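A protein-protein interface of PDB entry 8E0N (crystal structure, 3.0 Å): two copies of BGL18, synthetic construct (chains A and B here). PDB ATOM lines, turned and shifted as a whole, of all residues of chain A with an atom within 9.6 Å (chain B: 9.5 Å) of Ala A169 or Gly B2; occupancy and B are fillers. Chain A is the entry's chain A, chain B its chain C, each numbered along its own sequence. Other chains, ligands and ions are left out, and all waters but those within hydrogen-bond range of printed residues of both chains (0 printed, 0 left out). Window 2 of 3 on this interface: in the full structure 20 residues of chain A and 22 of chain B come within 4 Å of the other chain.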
ATOM      1  N   GLY A 116     -26.376 -10.536   3.105  1.00  0.00           N
ATOM      2  CA  GLY A 116     -27.021  -9.287   3.446  1.00  0.00           C
ATOM      3  C   GLY A 116     -27.339  -9.096   4.912  1.00  0.00           C
ATOM      4  O   GLY A 116     -27.933  -8.071   5.268  1.00  0.00           O
ATOM      5  N   PHE A 118     -26.249  -7.801   7.824  1.00  0.00           N
ATOM      6  CA  PHE A 118     -25.183  -6.918   8.279  1.00  0.00           C
ATOM      7  C   PHE A 118     -25.002  -6.949   9.790  1.00  0.00           C
ATOM      8  O   PHE A 118     -23.919  -6.611  10.279  1.00  0.00           O
ATOM      9  CB  PHE A 118     -25.460  -5.489   7.808  1.00  0.00           C
ATOM     10  CG  PHE A 118     -25.513  -5.346   6.312  1.00  0.00           C
ATOM     11  CD1 PHE A 118     -24.770  -6.186   5.498  1.00  0.00           C
ATOM     12  CD2 PHE A 118     -26.306  -4.377   5.720  1.00  0.00           C
ATOM     13  CE1 PHE A 118     -24.815  -6.062   4.123  1.00  0.00           C
ATOM     14  CE2 PHE A 118     -26.355  -4.248   4.344  1.00  0.00           C
ATOM     15  CZ  PHE A 118     -25.609  -5.092   3.545  1.00  0.00           C
ATOM     16  N   GLU A 119     -26.030  -7.352  10.541  1.00  0.00           N
ATOM     17  CA  GLU A 119     -25.896  -7.435  11.993  1.00  0.00           C
ATOM     18  C   GLU A 119     -24.942  -8.555  12.390  1.00  0.00           C
ATOM     19  O   GLU A 119     -24.041  -8.355  13.212  1.00  0.00           O
ATOM     20  CB  GLU A 119     -27.270  -7.642  12.634  1.00  0.00           C
ATOM     21  N   LEU A 122     -21.246  -7.616  11.609  1.00  0.00           N
ATOM     22  CA  LEU A 122     -20.589  -6.808  12.632  1.00  0.00           C
ATOM     23  C   LEU A 122     -20.369  -7.603  13.912  1.00  0.00           C
ATOM     24  O   LEU A 122     -19.369  -7.401  14.612  1.00  0.00           O
ATOM     25  CB  LEU A 122     -21.411  -5.548  12.906  1.00  0.00           C
ATOM     26  CG  LEU A 122     -21.674  -4.682  11.673  1.00  0.00           C
ATOM     27  CD1 LEU A 122     -22.797  -3.693  11.928  1.00  0.00           C
ATOM     28  CD2 LEU A 122     -20.402  -3.957  11.264  1.00  0.00           C
ATOM     29  N   TRP A 161     -13.839  -3.731   7.030  1.00  0.00           N
ATOM     30  CA  TRP A 161     -15.113  -4.336   6.662  1.00  0.00           C
ATOM     31  C   TRP A 161     -16.279  -3.686   7.394  1.00  0.00           C
ATOM     32  O   TRP A 161     -17.401  -3.675   6.877  1.00  0.00           O
ATOM     33  CB  TRP A 161     -15.086  -5.842   6.925  1.00  0.00           C
ATOM     34  CG  TRP A 161     -14.285  -6.605   5.912  1.00  0.00           C
ATOM     35  CD1 TRP A 161     -13.495  -6.080   4.931  1.00  0.00           C
ATOM     36  CD2 TRP A 161     -14.213  -8.028   5.766  1.00  0.00           C
ATOM     37  NE1 TRP A 161     -12.928  -7.087   4.189  1.00  0.00           N
ATOM     38  CE2 TRP A 161     -13.354  -8.293   4.680  1.00  0.00           C
ATOM     39  CE3 TRP A 161     -14.788  -9.105   6.447  1.00  0.00           C
ATOM     40  CZ2 TRP A 161     -13.055  -9.588   4.263  1.00  0.00           C
ATOM     41  CZ3 TRP A 161     -14.490 -10.390   6.031  1.00  0.00           C
ATOM     42  CH2 TRP A 161     -13.631 -10.621   4.949  1.00  0.00           C
ATOM     43  N   SER A 162     -16.040  -3.135   8.586  1.00  0.00           N
ATOM     44  CA  SER A 162     -17.106  -2.431   9.292  1.00  0.00           C
ATOM     45  C   SER A 162     -17.422  -1.099   8.624  1.00  0.00           C
ATOM     46  O   SER A 162     -18.590  -0.698   8.547  1.00  0.00           O
ATOM     47  CB  SER A 162     -16.718  -2.217  10.753  1.00  0.00           C
ATOM     48  OG  SER A 162     -16.622  -3.453  11.438  1.00  0.00           O
ATOM     49  N   ARG A 163     -16.392  -0.401   8.139  1.00  0.00           N
ATOM     50  CA  ARG A 163     -16.607   0.876   7.463  1.00  0.00           C
ATOM     51  C   ARG A 163     -17.459   0.705   6.213  1.00  0.00           C
ATOM     52  O   ARG A 163     -18.314   1.547   5.915  1.00  0.00           O
ATOM     53  CB  ARG A 163     -15.265   1.507   7.100  1.00  0.00           C
ATOM     54  CG  ARG A 163     -15.375   2.876   6.456  1.00  0.00           C
ATOM     55  CD  ARG A 163     -14.035   3.578   6.478  1.00  0.00           C
ATOM     56  NE  ARG A 163     -12.941   2.634   6.283  1.00  0.00           N
ATOM     57  CZ  ARG A 163     -11.725   2.781   6.791  1.00  0.00           C
ATOM     58  NH1 ARG A 163     -11.408   3.829   7.531  1.00  0.00           N
ATOM     59  NH2 ARG A 163     -10.805   1.850   6.551  1.00  0.00           N
ATOM     60  N   GLU A 164     -17.232  -0.375   5.465  1.00  0.00           N
ATOM     61  CA  GLU A 164     -18.023  -0.625   4.266  1.00  0.00           C
ATOM     62  C   GLU A 164     -19.487  -0.853   4.623  1.00  0.00           C
ATOM     63  O   GLU A 164     -20.388  -0.308   3.975  1.00  0.00           O
ATOM     64  CB  GLU A 164     -17.451  -1.825   3.513  1.00  0.00           C
ATOM     65  CG  GLU A 164     -16.031  -1.622   3.004  1.00  0.00           C
ATOM     66  CD  GLU A 164     -15.406  -2.906   2.484  1.00  0.00           C
ATOM     67  OE1 GLU A 164     -16.149  -3.885   2.263  1.00  0.00           O
ATOM     68  OE2 GLU A 164     -14.172  -2.938   2.297  1.00  0.00           O
ATOM     69  N   ILE A 165     -19.743  -1.649   5.664  1.00  0.00           N
ATOM     70  CA  ILE A 165     -21.111  -1.826   6.143  1.00  0.00           C
ATOM     71  C   ILE A 165     -21.658  -0.525   6.715  1.00  0.00           C
ATOM     72  O   ILE A 165     -22.874  -0.293   6.697  1.00  0.00           O
ATOM     73  CB  ILE A 165     -21.175  -2.966   7.176  1.00  0.00           C
ATOM     74  CG1 ILE A 165     -20.425  -4.195   6.660  1.00  0.00           C
ATOM     75  CG2 ILE A 165     -22.616  -3.319   7.501  1.00  0.00           C
ATOM     76  CD1 ILE A 165     -20.521  -5.390   7.573  1.00  0.00           C
ATOM     77  N   ALA A 166     -20.785   0.343   7.231  1.00  0.00           N
ATOM     78  CA  ALA A 166     -21.242   1.647   7.697  1.00  0.00           C
ATOM     79  C   ALA A 166     -21.723   2.504   6.532  1.00  0.00           C
ATOM     80  O   ALA A 166     -22.680   3.274   6.672  1.00  0.00           O
ATOM     81  CB  ALA A 166     -20.127   2.353   8.465  1.00  0.00           C
ATOM     82  N   GLU A 167     -21.074   2.378   5.373  1.00  0.00           N
ATOM     83  CA  GLU A 167     -21.520   3.098   4.185  1.00  0.00           C
ATOM     84  C   GLU A 167     -22.689   2.400   3.503  1.00  0.00           C
ATOM     85  O   GLU A 167     -23.502   3.061   2.848  1.00  0.00           O
ATOM     86  CB  GLU A 167     -20.359   3.262   3.200  1.00  0.00           C
ATOM     87  CG  GLU A 167     -19.180   4.051   3.750  1.00  0.00           C
ATOM     88  CD  GLU A 167     -19.530   5.499   4.051  1.00  0.00           C
ATOM     89  OE1 GLU A 167     -20.503   6.017   3.463  1.00  0.00           O
ATOM     90  OE2 GLU A 167     -18.831   6.118   4.879  1.00  0.00           O
ATOM     91  N   GLN A 168     -22.791   1.076   3.642  1.00  0.00           N
ATOM     92  CA  GLN A 168     -23.903   0.345   3.046  1.00  0.00           C
ATOM     93  C   GLN A 168     -25.218   0.584   3.776  1.00  0.00           C
ATOM     94  O   GLN A 168     -26.279   0.257   3.235  1.00  0.00           O
ATOM     95  CB  GLN A 168     -23.602  -1.156   3.024  1.00  0.00           C
ATOM     96  CG  GLN A 168     -22.500  -1.573   2.061  1.00  0.00           C
ATOM     97  CD  GLN A 168     -22.062  -3.015   2.261  1.00  0.00           C
ATOM     98  OE1 GLN A 168     -22.434  -3.659   3.242  1.00  0.00           O
ATOM     99  NE2 GLN A 168     -21.269  -3.528   1.327  1.00  0.00           N
ATOM    100  N   ALA A 169     -25.177   1.152   4.982  1.00  0.00           N
ATOM    101  CA  ALA A 169     -26.351   1.250   5.835  1.00  0.00           C
ATOM    102  C   ALA A 169     -26.793   2.680   6.109  1.00  0.00           C
ATOM    103  O   ALA A 169     -27.740   2.879   6.878  1.00  0.00           O
ATOM    104  CB  ALA A 169     -26.090   0.533   7.165  1.00  0.00           C
ATOM    105  N   ARG A 170     -26.148   3.679   5.510  1.00  0.00           N
ATOM    106  CA  ARG A 170     -26.530   5.058   5.769  1.00  0.00           C
ATOM    107  C   ARG A 170     -27.765   5.437   4.958  1.00  0.00           C
ATOM    108  O   ARG A 170     -28.117   4.792   3.968  1.00  0.00           O
ATOM    109  CB  ARG A 170     -25.388   6.024   5.444  1.00  0.00           C
ATOM    110  CG  ARG A 170     -24.972   6.057   3.983  1.00  0.00           C
ATOM    111  CD  ARG A 170     -23.701   6.874   3.798  1.00  0.00           C
ATOM    112  NE  ARG A 170     -23.948   8.292   4.033  1.00  0.00           N
ATOM    113  CZ  ARG A 170     -23.001   9.208   4.192  1.00  0.00           C
ATOM    114  NH1 ARG A 170     -23.297  10.483   4.384  1.00  0.00           N
ATOM    115  NH2 ARG A 170     -21.724   8.834   4.156  1.00  0.00           N
ATOM    116  N   LYS A 171     -28.426   6.506   5.389  1.00  0.00           N
ATOM    117  CA  LYS A 171     -29.597   6.984   4.671  1.00  0.00           C
ATOM    118  C   LYS A 171     -29.183   7.672   3.374  1.00  0.00           C
ATOM    119  O   LYS A 171     -28.066   8.176   3.242  1.00  0.00           O
ATOM    120  CB  LYS A 171     -30.410   7.946   5.539  1.00  0.00           C
ATOM    121  N   GLU A 172     -30.106   7.697   2.415  1.00  0.00           N
ATOM    122  CA  GLU A 172     -29.812   8.201   1.074  1.00  0.00           C
ATOM    123  C   GLU A 172     -30.098   9.704   1.005  1.00  0.00           C
ATOM    124  O   GLU A 172     -31.014  10.174   0.328  1.00  0.00           O
ATOM    125  CB  GLU A 172     -30.611   7.421   0.039  1.00  0.00           C
ATOM    126  CG  GLU A 172     -29.966   6.112  -0.379  1.00  0.00           C
ATOM    127  CD  GLU A 172     -30.693   5.447  -1.528  1.00  0.00           C
ATOM    128  OE1 GLU A 172     -31.528   6.119  -2.171  1.00  0.00           O
ATOM    129  OE2 GLU A 172     -30.432   4.253  -1.789  1.00  0.00           O
ATOM    130  N   GLY A 173     -29.275  10.461   1.726  1.00  0.00           N
ATOM    131  CA  GLY A 173     -29.407  11.907   1.772  1.00  0.00           C
ATOM    132  C   GLY A 173     -28.119  12.609   2.154  1.00  0.00           C
ATOM    133  O   GLY A 173     -27.170  11.971   2.616  1.00  0.00           O
ATOM    134  N   GLU B   1     -33.177   4.300   1.901  1.00  0.00           N
ATOM    135  CA  GLU B   1     -33.501   3.908   3.266  1.00  0.00           C
ATOM    136  C   GLU B   1     -32.407   3.021   3.843  1.00  0.00           C
ATOM    137  O   GLU B   1     -31.922   2.105   3.180  1.00  0.00           O
ATOM    138  CB  GLU B   1     -34.848   3.184   3.315  1.00  0.00           C
ATOM    139  N   GLY B   2     -32.021   3.300   5.083  1.00  0.00           N
ATOM    140  CA  GLY B   2     -30.994   2.518   5.739  1.00  0.00           C
ATOM    141  C   GLY B   2     -31.276   2.303   7.209  1.00  0.00           C
ATOM    142  O   GLY B   2     -32.409   2.478   7.666  1.00  0.00           O
ATOM    143  N   SER B   3     -30.245   1.929   7.959  1.00  0.00           N
ATOM    144  CA  SER B   3     -30.369   1.641   9.387  1.00  0.00           C
ATOM    145  C   SER B   3     -29.321   2.439  10.148  1.00  0.00           C
ATOM    146  O   SER B   3     -28.140   2.049  10.177  1.00  0.00           O
ATOM    147  CB  SER B   3     -30.219   0.150   9.660  1.00  0.00           C
ATOM    148  N   PRO B   4     -29.700   3.564  10.760  1.00  0.00           N
ATOM    149  CA  PRO B   4     -28.743   4.294  11.606  1.00  0.00           C
ATOM    150  C   PRO B   4     -28.211   3.466  12.760  1.00  0.00           C
ATOM    151  O   PRO B   4     -27.089   3.707  13.222  1.00  0.00           O
ATOM    152  CB  PRO B   4     -29.572   5.483  12.104  1.00  0.00           C
ATOM    153  CG  PRO B   4     -30.535   5.725  10.994  1.00  0.00           C
ATOM    154  CD  PRO B   4     -30.937   4.337  10.554  1.00  0.00           C
ATOM    155  N   ARG B   5     -28.995   2.503  13.252  1.00  0.00           N
ATOM    156  CA  ARG B   5     -28.506   1.622  14.306  1.00  0.00           C
ATOM    157  C   ARG B   5     -27.365   0.747  13.810  1.00  0.00           C
ATOM    158  O   ARG B   5     -26.482   0.372  14.592  1.00  0.00           O
ATOM    159  CB  ARG B   5     -29.650   0.759  14.840  1.00  0.00           C
ATOM    160  N   LEU B   6     -27.362   0.416  12.517  1.00  0.00           N
ATOM    161  CA  LEU B   6     -26.265  -0.356  11.945  1.00  0.00           C
ATOM    162  C   LEU B   6     -25.028   0.510  11.738  1.00  0.00           C
ATOM    163  O   LEU B   6     -23.901   0.049  11.953  1.00  0.00           O
ATOM    164  CB  LEU B   6     -26.707  -0.992  10.626  1.00  0.00           C
ATOM    165  CG  LEU B   6     -27.386  -2.360  10.742  1.00  0.00           C
ATOM    166  CD1 LEU B   6     -27.958  -2.797   9.400  1.00  0.00           C
ATOM    167  CD2 LEU B   6     -26.420  -3.406  11.289  1.00  0.00           C
ATOM    168  N   VAL B   7     -25.218   1.765  11.322  1.00  0.00           N
ATOM    169  CA  VAL B   7     -24.096   2.696  11.247  1.00  0.00           C
ATOM    170  C   VAL B   7     -23.480   2.883  12.627  1.00  0.00           C
ATOM    171  O   VAL B   7     -22.254   2.958  12.775  1.00  0.00           O
ATOM    172  CB  VAL B   7     -24.555   4.035  10.637  1.00  0.00           C
ATOM    173  CG1 VAL B   7     -23.371   4.968  10.446  1.00  0.00           C
ATOM    174  CG2 VAL B   7     -25.279   3.796   9.319  1.00  0.00           C
ATOM    175  N   LEU B   8     -24.323   2.953  13.659  1.00  0.00           N
ATOM    176  CA  LEU B   8     -23.845   2.952  15.037  1.00  0.00           C
ATOM    177  C   LEU B   8     -23.002   1.716  15.322  1.00  0.00           C
ATOM    178  O   LEU B   8     -21.828   1.815  15.697  1.00  0.00           O
ATOM    179  CB  LEU B   8     -25.036   3.004  15.991  1.00  0.00           C
ATOM    180  CG  LEU B   8     -25.286   4.231  16.862  1.00  0.00           C
ATOM    181  CD1 LEU B   8     -26.278   3.851  17.945  1.00  0.00           C
ATOM    182  CD2 LEU B   8     -23.997   4.752  17.465  1.00  0.00           C
ATOM    183  N   ARG B   9     -23.604   0.534  15.154  1.00  0.00           N
ATOM    184  CA  ARG B   9     -22.937  -0.723  15.475  1.00  0.00           C
ATOM    185  C   ARG B   9     -21.642  -0.889  14.692  1.00  0.00           C
ATOM    186  O   ARG B   9     -20.698  -1.522  15.179  1.00  0.00           O
ATOM    187  CB  ARG B   9     -23.898  -1.881  15.197  1.00  0.00           C
ATOM    188  CG  ARG B   9     -23.347  -3.285  15.401  1.00  0.00           C
ATOM    189  CD  ARG B   9     -22.785  -3.502  16.790  1.00  0.00           C
ATOM    190  NE  ARG B   9     -22.288  -4.864  16.941  1.00  0.00           N
ATOM    191  CZ  ARG B   9     -21.371  -5.237  17.822  1.00  0.00           C
ATOM    192  NH1 ARG B   9     -20.817  -4.368  18.651  1.00  0.00           N
ATOM    193  NH2 ARG B   9     -21.002  -6.514  17.874  1.00  0.00           N
ATOM    194  N   ALA B  10     -21.576  -0.326  13.484  1.00  0.00           N
ATOM    195  CA  ALA B  10     -20.341  -0.383  12.711  1.00  0.00           C
ATOM    196  C   ALA B  10     -19.279   0.535  13.304  1.00  0.00           C
ATOM    197  O   ALA B  10     -18.103   0.158  13.392  1.00  0.00           O
ATOM    198  CB  ALA B  10     -20.616  -0.018  11.254  1.00  0.00           C
ATOM    199  N   LEU B  11     -19.673   1.744  13.717  1.00  0.00           N
ATOM    200  CA  LEU B  11     -18.722   2.648  14.356  1.00  0.00           C
ATOM    201  C   LEU B  11     -18.227   2.091  15.683  1.00  0.00           C
ATOM    202  O   LEU B  11     -17.098   2.381  16.096  1.00  0.00           O
ATOM    203  CB  LEU B  11     -19.352   4.025  14.563  1.00  0.00           C
ATOM    204  CG  LEU B  11     -19.703   4.800  13.293  1.00  0.00           C
ATOM    205  CD1 LEU B  11     -20.393   6.114  13.629  1.00  0.00           C
ATOM    206  CD2 LEU B  11     -18.455   5.039  12.471  1.00  0.00           C
ATOM    207  N   LEU B  51     -22.747  11.818  12.973  1.00  0.00           N
ATOM    208  CA  LEU B  51     -23.944  11.040  13.278  1.00  0.00           C
ATOM    209  C   LEU B  51     -24.707  11.652  14.445  1.00  0.00           C
ATOM    210  O   LEU B  51     -25.937  11.766  14.400  1.00  0.00           O
ATOM    211  CB  LEU B  51     -23.563   9.583  13.567  1.00  0.00           C
ATOM    212  CG  LEU B  51     -24.600   8.467  13.364  1.00  0.00           C
ATOM    213  CD1 LEU B  51     -23.926   7.104  13.363  1.00  0.00           C
ATOM    214  CD2 LEU B  51     -25.695   8.495  14.419  1.00  0.00           C
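Of the printed residues of chain B, Ser A162 touches Ala B10. Arg A163 touches none of the printed residues of chain B. Ala A169 touches just these residues of chain B: Gly B2 (3.5 Å), Ser B3 (2.9 Å), Leu B6 (3.8 Å) and Val B7 (3.6 Å). Of the printed residues of chain B, Arg A170 touches Val B7 (3.9 Å). No residue of chain A comes within 4 Å of Glu B1. Of chain A, only Ala A169 (2.9 Å) comes within 4 Å of Ser B3. Of the printed residues of chain A, Val B7 touches Ala A166 (3.7 Å), Ala A169 (3.6 Å) and Arg A170 (3.9 Å). Of the printed residues of chain A, Ala B10 touches Leu A122, Ser A162 and Ala A166. The nearest residue of chain A that does not touch Gly B2 is Arg A170 (4.1 Å). The nearest printed residue of chain A that does not touch Val B7 is Ile A165 (5.4 Å).
The backbone carbonyl oxygen (O) of Ala A169 is in hydrogen-bond range of the backbone NH (N) of Ser B3 (2.9 Å).
No position is printed for both chains. Of the 11 pairs that touch across the chains among the printed residues, none has its exchanged pair printed and touching as well.
The side-chain carboxylate (OE1) of Glu A167 is in salt-bridge range of the guanidinium group (NH2) of Arg A170 (3.1 Å).
Of the 12 printed residues of chain B, 6 touch a printed residue of chain A. Along chain B the printed residues that touch a printed residue of chain A span positions 2 to 10. Of the 17 printed residues of chain A, 5 touch a printed residue of chain B. Among the printed residues, no Asp or Glu carboxylate lies within 4 Å of a Lys or Arg side-chain nitrogen of the other chain.
Among the printed residues, merely in contact across the chains: Leu A122 with Leu B6 (3.7 Å), Leu A122 with Arg B9 (3.5 Å), Leu A122 with Ala B10 (3.9 Å), Ser A162 with Ala B10 (3.4 Å), Ala A166 with Val B7 (3.7 Å), Ala A166 with Ala B10 (3.7 Å), Ala A169 with Gly B2 (3.5 Å), Ala A169 with Leu B6 (3.8 Å), Ala A169 with Val B7 (3.6 Å) and Arg A170 with Val B7 (3.9 Å).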
